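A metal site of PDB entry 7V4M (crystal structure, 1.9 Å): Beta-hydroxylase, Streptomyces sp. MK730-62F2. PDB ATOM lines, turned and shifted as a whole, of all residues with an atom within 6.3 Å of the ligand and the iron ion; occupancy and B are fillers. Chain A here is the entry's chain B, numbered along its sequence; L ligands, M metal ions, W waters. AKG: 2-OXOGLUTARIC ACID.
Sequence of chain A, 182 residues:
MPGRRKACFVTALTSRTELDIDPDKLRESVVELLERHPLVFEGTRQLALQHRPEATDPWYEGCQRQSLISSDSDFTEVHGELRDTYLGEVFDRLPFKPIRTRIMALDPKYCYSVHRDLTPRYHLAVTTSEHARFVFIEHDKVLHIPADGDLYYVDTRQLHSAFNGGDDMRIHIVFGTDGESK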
ATOM      1  N   THR A  44      -3.328  -5.784  21.323  1.00  0.00           N
ATOM      2  CA  THR A  44      -4.226  -4.722  21.741  1.00  0.00           C
ATOM      3  C   THR A  44      -3.379  -3.508  22.034  1.00  0.00           C
ATOM      4  O   THR A  44      -2.636  -3.479  23.026  1.00  0.00           O
ATOM      5  CB  THR A  44      -5.038  -5.094  22.985  1.00  0.00           C
ATOM      6  OG1 THR A  44      -5.676  -6.356  22.799  1.00  0.00           O
ATOM      7  CG2 THR A  44      -6.091  -4.019  23.233  1.00  0.00           C
ATOM      8  N   MET A 104      -8.615   1.712  22.821  1.00  0.00           N
ATOM      9  CA  MET A 104      -8.310   0.281  22.746  1.00  0.00           C
ATOM     10  C   MET A 104      -8.392  -0.127  21.287  1.00  0.00           C
ATOM     11  O   MET A 104      -9.462  -0.036  20.670  1.00  0.00           O
ATOM     12  CB  MET A 104      -9.278  -0.557  23.573  1.00  0.00           C
ATOM     13  CG  MET A 104      -9.403  -0.080  25.003  1.00  0.00           C
ATOM     14  SD  MET A 104      -8.041  -0.661  25.994  1.00  0.00           S
ATOM     15  CE  MET A 104      -8.703  -2.264  26.442  1.00  0.00           C
ATOM     16  N   ALA A 105      -7.263  -0.549  20.736  1.00  0.00           N
ATOM     17  CA  ALA A 105      -7.181  -0.853  19.314  1.00  0.00           C
ATOM     18  C   ALA A 105      -6.834  -2.328  19.151  1.00  0.00           C
ATOM     19  O   ALA A 105      -5.890  -2.818  19.790  1.00  0.00           O
ATOM     20  CB  ALA A 105      -6.132   0.026  18.651  1.00  0.00           C
ATOM     21  N   LEU A 106      -7.589  -3.022  18.317  1.00  0.00           N
ATOM     22  CA  LEU A 106      -7.312  -4.415  18.003  1.00  0.00           C
ATOM     23  C   LEU A 106      -6.627  -4.477  16.645  1.00  0.00           C
ATOM     24  O   LEU A 106      -7.170  -3.990  15.646  1.00  0.00           O
ATOM     25  CB  LEU A 106      -8.603  -5.246  17.983  1.00  0.00           C
ATOM     26  CG  LEU A 106      -9.302  -5.595  19.287  1.00  0.00           C
ATOM     27  CD1 LEU A 106     -10.418  -6.634  19.069  1.00  0.00           C
ATOM     28  CD2 LEU A 106      -8.292  -6.124  20.287  1.00  0.00           C
ATOM     29  N   TYR A 112      -9.028 -11.226  22.035  1.00  0.00           N
ATOM     30  CA  TYR A 112      -8.698 -11.275  23.455  1.00  0.00           C
ATOM     31  C   TYR A 112      -8.906 -12.670  24.021  1.00  0.00           C
ATOM     32  O   TYR A 112      -9.676 -13.480  23.489  1.00  0.00           O
ATOM     33  CB  TYR A 112      -9.593 -10.324  24.264  1.00  0.00           C
ATOM     34  CG  TYR A 112      -9.413  -8.854  24.017  1.00  0.00           C
ATOM     35  CD1 TYR A 112      -8.308  -8.191  24.518  1.00  0.00           C
ATOM     36  CD2 TYR A 112     -10.364  -8.139  23.311  1.00  0.00           C
ATOM     37  CE1 TYR A 112      -8.135  -6.823  24.293  1.00  0.00           C
ATOM     38  CE2 TYR A 112     -10.203  -6.764  23.085  1.00  0.00           C
ATOM     39  CZ  TYR A 112      -9.090  -6.128  23.594  1.00  0.00           C
ATOM     40  OH  TYR A 112      -8.942  -4.773  23.387  1.00  0.00           O
ATOM     41  N   SER A 113      -8.303 -12.922  25.172  1.00  0.00           N
ATOM     42  CA  SER A 113      -8.692 -14.106  25.905  1.00  0.00           C
ATOM     43  C   SER A 113     -10.160 -14.002  26.341  1.00  0.00           C
ATOM     44  O   SER A 113     -10.743 -12.923  26.355  1.00  0.00           O
ATOM     45  CB  SER A 113      -7.795 -14.285  27.135  1.00  0.00           C
ATOM     46  OG  SER A 113      -7.982 -13.201  28.013  1.00  0.00           O
ATOM     47  N   HIS A 115     -12.518 -13.850  29.186  1.00  0.00           N
ATOM     48  CA  HIS A 115     -12.199 -13.390  30.529  1.00  0.00           C
ATOM     49  C   HIS A 115     -13.366 -12.588  31.109  1.00  0.00           C
ATOM     50  O   HIS A 115     -14.360 -12.299  30.442  1.00  0.00           O
ATOM     51  CB  HIS A 115     -10.957 -12.505  30.519  1.00  0.00           C
ATOM     52  CG  HIS A 115     -11.157 -11.222  29.798  1.00  0.00           C
ATOM     53  ND1 HIS A 115     -11.193 -11.142  28.418  1.00  0.00           N
ATOM     54  CD2 HIS A 115     -11.389  -9.962  30.250  1.00  0.00           C
ATOM     55  CE1 HIS A 115     -11.425  -9.892  28.049  1.00  0.00           C
ATOM     56  NE2 HIS A 115     -11.546  -9.160  29.149  1.00  0.00           N
ATOM     57  N   ARG A 116     -13.229 -12.234  32.385  1.00  0.00           N
ATOM     58  CA  ARG A 116     -14.111 -11.320  33.077  1.00  0.00           C
ATOM     59  C   ARG A 116     -13.312 -10.122  33.562  1.00  0.00           C
ATOM     60  O   ARG A 116     -12.142 -10.265  33.925  1.00  0.00           O
ATOM     61  CB  ARG A 116     -14.803 -11.968  34.289  1.00  0.00           C
ATOM     62  CG  ARG A 116     -15.697 -13.150  34.004  1.00  0.00           C
ATOM     63  CD  ARG A 116     -16.111 -13.801  35.342  1.00  0.00           C
ATOM     64  NE  ARG A 116     -16.800 -15.066  35.113  1.00  0.00           N
ATOM     65  CZ  ARG A 116     -18.103 -15.180  34.912  1.00  0.00           C
ATOM     66  NH1 ARG A 116     -18.872 -14.091  34.899  1.00  0.00           N
ATOM     67  NH2 ARG A 116     -18.646 -16.371  34.700  1.00  0.00           N
ATOM     68  N   ASP A 117     -13.949  -8.957  33.548  1.00  0.00           N
ATOM     69  CA  ASP A 117     -13.367  -7.765  34.133  1.00  0.00           C
ATOM     70  C   ASP A 117     -14.079  -7.457  35.443  1.00  0.00           C
ATOM     71  O   ASP A 117     -15.131  -8.014  35.757  1.00  0.00           O
ATOM     72  CB  ASP A 117     -13.483  -6.571  33.193  1.00  0.00           C
ATOM     73  CG  ASP A 117     -12.691  -6.776  31.913  1.00  0.00           C
ATOM     74  OD1 ASP A 117     -11.447  -6.858  31.950  1.00  0.00           O
ATOM     75  OD2 ASP A 117     -13.326  -6.837  30.861  1.00  0.00           O
ATOM     76  N   THR A 119     -15.394  -4.521  36.444  1.00  0.00           N
ATOM     77  CA  THR A 119     -16.524  -3.630  36.263  1.00  0.00           C
ATOM     78  C   THR A 119     -17.014  -3.689  34.828  1.00  0.00           C
ATOM     79  O   THR A 119     -16.284  -4.149  33.941  1.00  0.00           O
ATOM     80  CB  THR A 119     -16.138  -2.177  36.612  1.00  0.00           C
ATOM     81  OG1 THR A 119     -15.287  -1.640  35.597  1.00  0.00           O
ATOM     82  CG2 THR A 119     -15.388  -2.119  37.953  1.00  0.00           C
ATOM     83  N   ARG A 121     -18.263  -1.649  31.271  1.00  0.00           N
ATOM     84  CA  ARG A 121     -17.593  -0.620  30.487  1.00  0.00           C
ATOM     85  C   ARG A 121     -18.500  -0.158  29.374  1.00  0.00           C
ATOM     86  O   ARG A 121     -19.391  -0.890  28.933  1.00  0.00           O
ATOM     87  CB  ARG A 121     -16.282  -1.139  29.873  1.00  0.00           C
ATOM     88  CG  ARG A 121     -15.266  -1.578  30.887  1.00  0.00           C
ATOM     89  CD  ARG A 121     -14.158  -2.382  30.274  1.00  0.00           C
ATOM     90  NE  ARG A 121     -13.107  -2.606  31.261  1.00  0.00           N
ATOM     91  CZ  ARG A 121     -11.925  -3.144  30.990  1.00  0.00           C
ATOM     92  NH1 ARG A 121     -11.044  -3.320  31.957  1.00  0.00           N
ATOM     93  NH2 ARG A 121     -11.633  -3.519  29.746  1.00  0.00           N
ATOM     94  N   HIS A 123     -18.382   1.325  25.375  1.00  0.00           N
ATOM     95  CA  HIS A 123     -17.603   1.458  24.144  1.00  0.00           C
ATOM     96  C   HIS A 123     -18.188   2.533  23.240  1.00  0.00           C
ATOM     97  O   HIS A 123     -19.406   2.606  23.023  1.00  0.00           O
ATOM     98  CB  HIS A 123     -17.538   0.146  23.364  1.00  0.00           C
ATOM     99  CG  HIS A 123     -16.731  -0.919  24.050  1.00  0.00           C
ATOM    100  ND1 HIS A 123     -15.680  -1.547  23.436  1.00  0.00           N
ATOM    101  CD2 HIS A 123     -16.819  -1.428  25.293  1.00  0.00           C
ATOM    102  CE1 HIS A 123     -15.137  -2.413  24.284  1.00  0.00           C
ATOM    103  NE2 HIS A 123     -15.819  -2.357  25.411  1.00  0.00           N
ATOM    104  N   PHE A 134     -18.050  -8.464  19.558  1.00  0.00           N
ATOM    105  CA  PHE A 134     -17.916  -8.665  20.991  1.00  0.00           C
ATOM    106  C   PHE A 134     -18.773  -9.880  21.323  1.00  0.00           C
ATOM    107  O   PHE A 134     -19.902  -9.982  20.837  1.00  0.00           O
ATOM    108  CB  PHE A 134     -18.367  -7.385  21.694  1.00  0.00           C
ATOM    109  CG  PHE A 134     -18.133  -7.372  23.163  1.00  0.00           C
ATOM    110  CD1 PHE A 134     -19.005  -8.042  24.009  1.00  0.00           C
ATOM    111  CD2 PHE A 134     -17.082  -6.647  23.707  1.00  0.00           C
ATOM    112  CE1 PHE A 134     -18.808  -8.027  25.399  1.00  0.00           C
ATOM    113  CE2 PHE A 134     -16.880  -6.623  25.083  1.00  0.00           C
ATOM    114  CZ  PHE A 134     -17.750  -7.303  25.932  1.00  0.00           C
ATOM    115  N   ILE A 145     -20.365  -3.580  17.676  1.00  0.00           N
ATOM    116  CA  ILE A 145     -20.467  -2.208  18.148  1.00  0.00           C
ATOM    117  C   ILE A 145     -20.154  -1.284  16.977  1.00  0.00           C
ATOM    118  O   ILE A 145     -18.968  -1.156  16.602  1.00  0.00           O
ATOM    119  CB  ILE A 145     -19.539  -1.941  19.345  1.00  0.00           C
ATOM    120  CG1 ILE A 145     -19.985  -2.822  20.525  1.00  0.00           C
ATOM    121  CG2 ILE A 145     -19.564  -0.435  19.723  1.00  0.00           C
ATOM    122  CD1 ILE A 145     -18.982  -2.919  21.640  1.00  0.00           C
ATOM    123  N   VAL A 154     -21.504  -2.572  27.821  1.00  0.00           N
ATOM    124  CA  VAL A 154     -21.357  -4.023  27.862  1.00  0.00           C
ATOM    125  C   VAL A 154     -20.980  -4.410  29.290  1.00  0.00           C
ATOM    126  O   VAL A 154     -20.035  -3.866  29.853  1.00  0.00           O
ATOM    127  CB  VAL A 154     -20.302  -4.556  26.870  1.00  0.00           C
ATOM    128  CG1 VAL A 154     -20.847  -4.569  25.462  1.00  0.00           C
ATOM    129  CG2 VAL A 154     -19.050  -3.706  26.923  1.00  0.00           C
ATOM    130  N   THR A 156     -19.064  -6.290  31.129  1.00  0.00           N
ATOM    131  CA  THR A 156     -17.855  -7.098  30.977  1.00  0.00           C
ATOM    132  C   THR A 156     -17.493  -7.847  32.252  1.00  0.00           C
ATOM    133  O   THR A 156     -16.430  -8.480  32.303  1.00  0.00           O
ATOM    134  CB  THR A 156     -16.705  -6.207  30.505  1.00  0.00           C
ATOM    135  OG1 THR A 156     -16.679  -5.003  31.271  1.00  0.00           O
ATOM    136  CG2 THR A 156     -16.905  -5.860  29.040  1.00  0.00           C
ATOM    137  N   HIS A 160     -16.533 -12.984  28.513  1.00  0.00           N
ATOM    138  CA  HIS A 160     -16.577 -12.384  27.179  1.00  0.00           C
ATOM    139  C   HIS A 160     -15.204 -12.421  26.517  1.00  0.00           C
ATOM    140  O   HIS A 160     -14.174 -12.669  27.144  1.00  0.00           O
ATOM    141  CB  HIS A 160     -17.079 -10.920  27.244  1.00  0.00           C
ATOM    142  CG  HIS A 160     -16.120  -9.990  27.932  1.00  0.00           C
ATOM    143  ND1 HIS A 160     -16.036  -9.900  29.306  1.00  0.00           N
ATOM    144  CD2 HIS A 160     -15.197  -9.141  27.435  1.00  0.00           C
ATOM    145  CE1 HIS A 160     -15.105  -9.029  29.626  1.00  0.00           C
ATOM    146  NE2 HIS A 160     -14.580  -8.538  28.508  1.00  0.00           N
ATOM    147  N   SER A 161     -15.226 -12.170  25.209  1.00  0.00           N
ATOM    148  CA  SER A 161     -14.046 -11.816  24.440  1.00  0.00           C
ATOM    149  C   SER A 161     -14.486 -10.809  23.375  1.00  0.00           C
ATOM    150  O   SER A 161     -15.667 -10.502  23.250  1.00  0.00           O
ATOM    151  CB  SER A 161     -13.386 -13.067  23.811  1.00  0.00           C
ATOM    152  OG  SER A 161     -12.235 -12.692  23.071  1.00  0.00           O
ATOM    153  N   ALA A 162     -13.533 -10.286  22.623  1.00  0.00           N
ATOM    154  CA  ALA A 162     -13.824  -9.473  21.444  1.00  0.00           C
ATOM    155  C   ALA A 162     -12.780  -9.798  20.403  1.00  0.00           C
ATOM    156  O   ALA A 162     -11.668 -10.207  20.738  1.00  0.00           O
ATOM    157  CB  ALA A 162     -13.822  -7.968  21.754  1.00  0.00           C
ATOM    158  N   ARG A 170      -9.138  -2.096  14.487  1.00  0.00           N
ATOM    159  CA  ARG A 170     -10.448  -1.762  15.040  1.00  0.00           C
ATOM    160  C   ARG A 170     -10.206  -0.910  16.288  1.00  0.00           C
ATOM    161  O   ARG A 170      -9.658  -1.389  17.273  1.00  0.00           O
ATOM    162  CB  ARG A 170     -11.234  -3.037  15.357  1.00  0.00           C
ATOM    163  CG  ARG A 170     -12.618  -2.807  15.953  1.00  0.00           C
ATOM    164  CD  ARG A 170     -12.774  -3.514  17.277  1.00  0.00           C
ATOM    165  NE  ARG A 170     -11.972  -2.921  18.333  1.00  0.00           N
ATOM    166  CZ  ARG A 170     -12.061  -3.204  19.626  1.00  0.00           C
ATOM    167  NH1 ARG A 170     -11.273  -2.576  20.505  1.00  0.00           N
ATOM    168  NH2 ARG A 170     -12.925  -4.121  20.048  1.00  0.00           N
ATOM    169  N   HIS A 172     -11.594   1.432  19.379  1.00  0.00           N
ATOM    170  CA  HIS A 172     -12.663   1.897  20.245  1.00  0.00           C
ATOM    171  C   HIS A 172     -12.085   2.836  21.297  1.00  0.00           C
ATOM    172  O   HIS A 172     -10.916   2.745  21.655  1.00  0.00           O
ATOM    173  CB  HIS A 172     -13.366   0.747  21.007  1.00  0.00           C
ATOM    174  CG  HIS A 172     -14.178  -0.170  20.144  1.00  0.00           C
ATOM    175  ND1 HIS A 172     -15.012  -1.127  20.669  1.00  0.00           N
ATOM    176  CD2 HIS A 172     -14.271  -0.286  18.800  1.00  0.00           C
ATOM    177  CE1 HIS A 172     -15.599  -1.785  19.682  1.00  0.00           C
ATOM    178  NE2 HIS A 172     -15.161  -1.301  18.539  1.00  0.00           N
ATOM    179  N   VAL A 174     -12.910   3.176  25.224  1.00  0.00           N
ATOM    180  CA  VAL A 174     -13.544   2.318  26.226  1.00  0.00           C
ATOM    181  C   VAL A 174     -13.519   3.056  27.575  1.00  0.00           C
ATOM    182  O   VAL A 174     -12.438   3.312  28.127  1.00  0.00           O
ATOM    183  CB  VAL A 174     -12.841   0.957  26.320  1.00  0.00           C
ATOM    184  CG1 VAL A 174     -13.486   0.085  27.402  1.00  0.00           C
ATOM    185  CG2 VAL A 174     -12.900   0.257  24.944  1.00  0.00           C
HETATM  186  C1  AKG L   1     -13.693  -5.047  27.491  1.00  0.00           C
HETATM  187  O1  AKG L   1     -13.637  -5.303  28.710  1.00  0.00           O
HETATM  188  O2  AKG L   1     -14.289  -4.008  27.075  1.00  0.00           O
HETATM  189  C2  AKG L   1     -12.979  -5.988  26.529  1.00  0.00           C
HETATM  190  O5  AKG L   1     -12.372  -6.998  26.924  1.00  0.00           O
HETATM  191  C3  AKG L   1     -13.023  -5.606  25.049  1.00  0.00           C
HETATM  192  C4  AKG L   1     -12.065  -4.425  24.859  1.00  0.00           C
HETATM  193  C5  AKG L   1     -12.106  -4.037  23.398  1.00  0.00           C
HETATM  194  O3  AKG L   1     -13.158  -4.287  22.796  1.00  0.00           O
HETATM  195  O4  AKG L   1     -11.049  -3.614  22.891  1.00  0.00           O
HETATM  196 FE    FE M   1     -12.726  -7.233  28.909  1.00  0.00          FE
HETATM  197  O   HOH W   1     -10.833  -6.294  29.255  1.00  0.00           O
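Merely in contact with the iron ion: Arg 121 (3.96 Å).
Of the 22 residues printed, 4 come within 4 Å of the iron ion.
Along chain A the residues within 4 Å of the iron ion span positions 115 to 160.
The nearest printed residue that does not touch the iron ion is Thr 156 (4.4 Å).
Water W1 bridges the side-chain carboxylate (OD1) of Asp 117 (2.8 Å) and the guanidinium group (NH2) of Arg 121 (2.9 Å).
An oxygen (O4) of the ligand is in hydrogen-bond range of the side-chain hydroxyl of Tyr 112.
An oxygen (O4) of the ligand lies within salt-bridge range of the guanidinium group of Arg 170.
NE2 of His 123 sits at hydrogen-bond distance from O2 of the ligand, at 2.8 Å.
The guanidinium group (NH2) of Arg 121 lies within salt-bridge range of an oxygen (O2) of the ligand (3.8 Å).
O5 of the ligand binds the iron ion (2.0 Å).
OD2 of Asp 117 binds the iron ion, 2.1 Å away.
The iron ion is bound by water W1 (2.1 Å).
O1 of the ligand is bound to the iron ion (2.1 Å).
The iron ion is bound by NE2 of His 115 (2.3 Å).
The iron ion is bound by NE2 of His 160 (2.3 Å).
The iron ion has six donor atoms within binding distance.
Merely in contact with the ligand: Thr 156, Met 104, Ala 162 and Phe 134.
Hydrophobic or aromatic side chains within 4 Å of the ligand: Met 104, Tyr 112, His 115, His 123, Phe 134, His 160 and Ala 162.
Along chain A the residues within 4 Å of the ligand span positions 104 to 170.
The guanidinium group of Arg 121 is in salt-bridge range of the side-chain carboxylate of Asp 117, at 3.6 Å.
A ring nitrogen (ND1) of His 115 lies within hydrogen-bond range of the backbone carbonyl oxygen (O) of Ser 113 (2.8 Å).
ND1 of His 160 lies close to O of Thr 156 (3.3 Å).
NH1 of Arg 170 lies within hydrogen-bond range of O of Met 104 (3.1 Å).
ND1 of His 172 lies within hydrogen-bond range of ND1 of His 123, 2.9 Å away.
The backbone NH (N) of Val 154 is in hydrogen-bond range of the backbone carbonyl oxygen (O) of Arg 121, at 2.9 Å.
The backbone carbonyl oxygen (O) of Thr 119 is in hydrogen-bond range of the side-chain hydroxyl (OG1) of Thr 156, at 2.8 Å.
The backbone NH (N) of Met 104 sits at hydrogen-bond distance from the backbone carbonyl oxygen (O) of His 172, 2.8 Å away.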
